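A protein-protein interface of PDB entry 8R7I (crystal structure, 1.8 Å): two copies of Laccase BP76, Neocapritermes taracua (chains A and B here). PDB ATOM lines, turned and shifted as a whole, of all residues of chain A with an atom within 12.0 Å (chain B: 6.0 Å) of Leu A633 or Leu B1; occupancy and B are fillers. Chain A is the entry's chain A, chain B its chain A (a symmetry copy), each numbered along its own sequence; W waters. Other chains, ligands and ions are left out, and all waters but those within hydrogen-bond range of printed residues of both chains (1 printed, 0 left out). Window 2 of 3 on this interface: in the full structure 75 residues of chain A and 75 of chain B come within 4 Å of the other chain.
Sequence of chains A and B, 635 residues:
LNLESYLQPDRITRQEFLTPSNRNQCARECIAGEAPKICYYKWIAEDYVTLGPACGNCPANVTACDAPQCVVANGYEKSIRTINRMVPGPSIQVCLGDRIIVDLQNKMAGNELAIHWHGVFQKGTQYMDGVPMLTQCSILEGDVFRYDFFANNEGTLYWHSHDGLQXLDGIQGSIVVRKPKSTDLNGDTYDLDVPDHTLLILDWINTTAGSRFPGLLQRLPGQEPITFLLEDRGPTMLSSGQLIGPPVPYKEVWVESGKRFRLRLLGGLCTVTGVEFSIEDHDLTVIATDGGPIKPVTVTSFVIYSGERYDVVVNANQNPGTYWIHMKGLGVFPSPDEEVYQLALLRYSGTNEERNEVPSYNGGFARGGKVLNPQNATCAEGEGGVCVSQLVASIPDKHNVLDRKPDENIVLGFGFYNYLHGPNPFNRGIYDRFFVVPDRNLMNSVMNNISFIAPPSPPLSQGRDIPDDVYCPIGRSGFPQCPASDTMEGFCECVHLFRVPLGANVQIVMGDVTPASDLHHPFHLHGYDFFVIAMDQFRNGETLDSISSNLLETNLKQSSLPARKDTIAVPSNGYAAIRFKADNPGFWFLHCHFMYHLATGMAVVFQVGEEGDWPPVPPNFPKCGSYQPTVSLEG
O of Ser A632 sits at hydrogen-bond distance from NH1 of Arg B99, 2.9 Å away.
No position is printed for both chains.
Of the 7 pairs that touch across the chains among the printed residues, none has its exchanged pair printed and touching as well.
Among the printed residues, pairs that only touch across the chains: Leu A633 with Ile B38, Val A631 with Leu B1, Val A631 with Arg B99, Leu A633 with Leu B1, Ser A632 with Leu B1 and Val A631 with Leu B3.
Pro A629 touches none of the printed residues of chain B.
Of the printed residues of chain B, Val A631 touches Leu B1, Leu B3 and Arg B99.
Of the printed residues of chain A, Leu B1 touches Val A631 (3.6 Å), Ser A632 (3.8 Å) and Leu A633 (3.6 Å).
Asn B2 touches none of the printed residues of chain A.
Of chain A, only Val A631 (3.9 Å) comes within 4 Å of Leu B3.
Of the printed residues of chain A, Ile B38 touches Leu A633 (3.6 Å).
Of the printed residues of chain A, Arg B99 touches Val A631 and Ser A632.
The nearest residue of chain B that does not touch Leu A633 is Arg B99 (4.7 Å).
The nearest printed residue of chain B that does not touch Val A631 is Ile B38 (5.1 Å).
Of the 6 printed residues of chain A, 3 touch a printed residue of chain B.
Hydrophobic or aromatic side chains of chain A within 4 Å of the printed part of chain B: Val A631 and Leu A633.
Of the 6 printed residues of chain B, 4 touch a printed residue of chain A.
Printed residues of chain B that touch a printed residue of chain A: Leu B1, Leu B3, Ile B38 and Arg B99.
Among the printed residues, 7 pairs touch across the chains.
Among the printed residues, no Asp or Glu carboxylate lies within 4 Å of a Lys or Arg side-chain nitrogen of the other chain.
Water W1 lies within hydrogen-bond range of the backbone NH of Ser A632 (2.7 Å), the guanidinium group of Arg B99 (3.0 Å) and the backbone carbonyl oxygen of Thr A630 (3.4 Å).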
ATOM      1  N   GLN A 628       5.696  25.310   7.224  1.00  0.00           N
ATOM      2  CA  GLN A 628       5.046  24.761   8.410  1.00  0.00           C
ATOM      3  C   GLN A 628       5.080  23.236   8.352  1.00  0.00           C
ATOM      4  O   GLN A 628       4.053  22.617   8.124  1.00  0.00           O
ATOM      5  CB  GLN A 628       3.627  25.304   8.492  1.00  0.00           C
ATOM      6  CG  GLN A 628       3.619  26.785   8.852  1.00  0.00           C
ATOM      7  CD  GLN A 628       2.202  27.251   9.006  1.00  0.00           C
ATOM      8  OE1 GLN A 628       1.479  27.380   8.042  1.00  0.00           O
ATOM      9  NE2 GLN A 628       1.803  27.477  10.236  1.00  0.00           N
ATOM     10  N   PRO A 629       6.245  22.596   8.539  1.00  0.00           N
ATOM     11  CA  PRO A 629       6.314  21.135   8.512  1.00  0.00           C
ATOM     12  C   PRO A 629       5.461  20.524   9.634  1.00  0.00           C
ATOM     13  O   PRO A 629       5.429  21.029  10.764  1.00  0.00           O
ATOM     14  CB  PRO A 629       7.781  20.794   8.820  1.00  0.00           C
ATOM     15  CG  PRO A 629       8.535  22.081   8.578  1.00  0.00           C
ATOM     16  CD  PRO A 629       7.544  23.211   8.810  1.00  0.00           C
ATOM     17  N   THR A 630       4.773  19.430   9.290  1.00  0.00           N
ATOM     18  CA  THR A 630       4.013  18.623  10.247  1.00  0.00           C
ATOM     19  C   THR A 630       4.881  18.299  11.458  1.00  0.00           C
ATOM     20  O   THR A 630       6.011  17.844  11.301  1.00  0.00           O
ATOM     21  CB  THR A 630       3.510  17.334   9.587  1.00  0.00           C
ATOM     22  OG1 THR A 630       2.634  17.807   8.559  1.00  0.00           O
ATOM     23  CG2 THR A 630       2.809  16.415  10.554  1.00  0.00           C
ATOM     24  N   VAL A 631       4.348  18.562  12.662  1.00  0.00           N
ATOM     25  CA  VAL A 631       4.969  18.180  13.924  1.00  0.00           C
ATOM     26  C   VAL A 631       4.483  16.766  14.319  1.00  0.00           C
ATOM     27  O   VAL A 631       3.264  16.570  14.424  1.00  0.00           O
ATOM     28  CB  VAL A 631       4.631  19.216  15.011  1.00  0.00           C
ATOM     29  CG1 VAL A 631       5.187  18.819  16.376  1.00  0.00           C
ATOM     30  CG2 VAL A 631       5.124  20.602  14.612  1.00  0.00           C
ATOM     31  N   SER A 632       5.437  15.822  14.485  1.00  0.00           N
ATOM     32  CA  SER A 632       5.230  14.483  15.063  1.00  0.00           C
ATOM     33  C   SER A 632       5.986  14.378  16.401  1.00  0.00           C
ATOM     34  O   SER A 632       6.896  15.177  16.629  1.00  0.00           O
ATOM     35  CB  SER A 632       5.724  13.392  14.110  1.00  0.00           C
ATOM     36  OG  SER A 632       5.107  13.492  12.838  1.00  0.00           O
ATOM     37  N   LEU A 633       5.626  13.388  17.241  1.00  0.00           N
ATOM     38  CA  LEU A 633       6.419  12.931  18.391  1.00  0.00           C
ATOM     39  C   LEU A 633       7.561  12.027  17.886  1.00  0.00           C
ATOM     40  O   LEU A 633       8.749  12.446  17.939  1.00  0.00           O
ATOM     41  CB  LEU A 633       5.516  12.141  19.350  1.00  0.00           C
ATOM     42  CG  LEU A 633       4.381  12.930  19.999  1.00  0.00           C
ATOM     43  CD1 LEU A 633       3.340  11.992  20.608  1.00  0.00           C
ATOM     44  CD2 LEU A 633       4.923  13.880  21.056  1.00  0.00           C
ATOM     45  N   LEU B   1       0.145  15.142  15.695  1.00  0.00           N
ATOM     46  CA  LEU B   1      -0.159  15.934  16.918  1.00  0.00           C
ATOM     47  C   LEU B   1      -1.210  16.998  16.603  1.00  0.00           C
ATOM     48  O   LEU B   1      -1.197  17.564  15.501  1.00  0.00           O
ATOM     49  CB  LEU B   1       1.123  16.606  17.423  1.00  0.00           C
ATOM     50  CG  LEU B   1       2.125  15.678  18.106  1.00  0.00           C
ATOM     51  CD1 LEU B   1       3.435  16.392  18.363  1.00  0.00           C
ATOM     52  CD2 LEU B   1       1.546  15.120  19.400  1.00  0.00           C
ATOM     53  N   ASN B   2      -2.092  17.286  17.577  1.00  0.00           N
ATOM     54  CA  ASN B   2      -2.851  18.536  17.589  1.00  0.00           C
ATOM     55  C   ASN B   2      -1.999  19.598  18.320  1.00  0.00           C
ATOM     56  O   ASN B   2      -2.061  19.683  19.556  1.00  0.00           O
ATOM     57  CB  ASN B   2      -4.236  18.371  18.227  1.00  0.00           C
ATOM     58  CG  ASN B   2      -5.028  19.662  18.231  1.00  0.00           C
ATOM     59  OD1 ASN B   2      -4.880  20.491  17.326  1.00  0.00           O
ATOM     60  ND2 ASN B   2      -5.846  19.853  19.256  1.00  0.00           N
ATOM     61  N   LEU B   3      -1.267  20.423  17.550  1.00  0.00           N
ATOM     62  CA  LEU B   3      -0.409  21.476  18.080  1.00  0.00           C
ATOM     63  C   LEU B   3      -1.159  22.426  19.011  1.00  0.00           C
ATOM     64  O   LEU B   3      -0.567  22.931  19.977  1.00  0.00           O
ATOM     65  CB  LEU B   3       0.195  22.286  16.937  1.00  0.00           C
ATOM     66  CG  LEU B   3       1.593  21.908  16.508  1.00  0.00           C
ATOM     67  CD1 LEU B   3       2.008  22.776  15.332  1.00  0.00           C
ATOM     68  CD2 LEU B   3       2.577  22.054  17.650  1.00  0.00           C
ATOM     69  N   TYR B   6      -0.994  22.183  22.722  1.00  0.00           N
ATOM     70  CA  TYR B   6       0.271  22.577  23.363  1.00  0.00           C
ATOM     71  C   TYR B   6       0.465  24.089  23.367  1.00  0.00           C
ATOM     72  O   TYR B   6       1.553  24.554  23.737  1.00  0.00           O
ATOM     73  CB  TYR B   6       1.447  21.883  22.678  1.00  0.00           C
ATOM     74  CG  TYR B   6       1.321  20.390  22.640  1.00  0.00           C
ATOM     75  CD1 TYR B   6       1.401  19.632  23.797  1.00  0.00           C
ATOM     76  CD2 TYR B   6       1.061  19.733  21.451  1.00  0.00           C
ATOM     77  CE1 TYR B   6       1.269  18.238  23.772  1.00  0.00           C
ATOM     78  CE2 TYR B   6       0.914  18.347  21.406  1.00  0.00           C
ATOM     79  CZ  TYR B   6       1.017  17.602  22.570  1.00  0.00           C
ATOM     80  OH  TYR B   6       0.902  16.251  22.498  1.00  0.00           O
ATOM     81  N   ILE B  38       6.141  19.595  24.898  1.00  0.00           N
ATOM     82  CA  ILE B  38       6.086  20.363  23.655  1.00  0.00           C
ATOM     83  C   ILE B  38       5.464  21.696  24.008  1.00  0.00           C
ATOM     84  O   ILE B  38       4.334  21.741  24.530  1.00  0.00           O
ATOM     85  CB  ILE B  38       5.280  19.599  22.586  1.00  0.00           C
ATOM     86  CG1 ILE B  38       5.969  18.265  22.284  1.00  0.00           C
ATOM     87  CG2 ILE B  38       5.106  20.450  21.329  1.00  0.00           C
ATOM     88  CD1 ILE B  38       5.220  17.447  21.255  1.00  0.00           C
ATOM     89  N   ARG B  99      10.680  21.002  23.988  1.00  0.00           N
ATOM     90  CA  ARG B  99      10.668  21.348  22.570  1.00  0.00           C
ATOM     91  C   ARG B  99       9.900  22.648  22.373  1.00  0.00           C
ATOM     92  O   ARG B  99       8.777  22.797  22.921  1.00  0.00           O
ATOM     93  CB  ARG B  99      10.025  20.203  21.781  1.00  0.00           C
ATOM     94  CG  ARG B  99      10.069  20.379  20.282  1.00  0.00           C
ATOM     95  CD  ARG B  99       9.489  19.125  19.656  1.00  0.00           C
ATOM     96  NE  ARG B  99       9.429  19.204  18.217  1.00  0.00           N
ATOM     97  CZ  ARG B  99       8.849  18.271  17.455  1.00  0.00           C
ATOM     98  NH1 ARG B  99       8.339  17.192  18.037  1.00  0.00           N
ATOM     99  NH2 ARG B  99       8.756  18.427  16.139  1.00  0.00           N
HETATM  100  O   HOH W   1       7.937  16.667  13.900  1.00  0.00           O
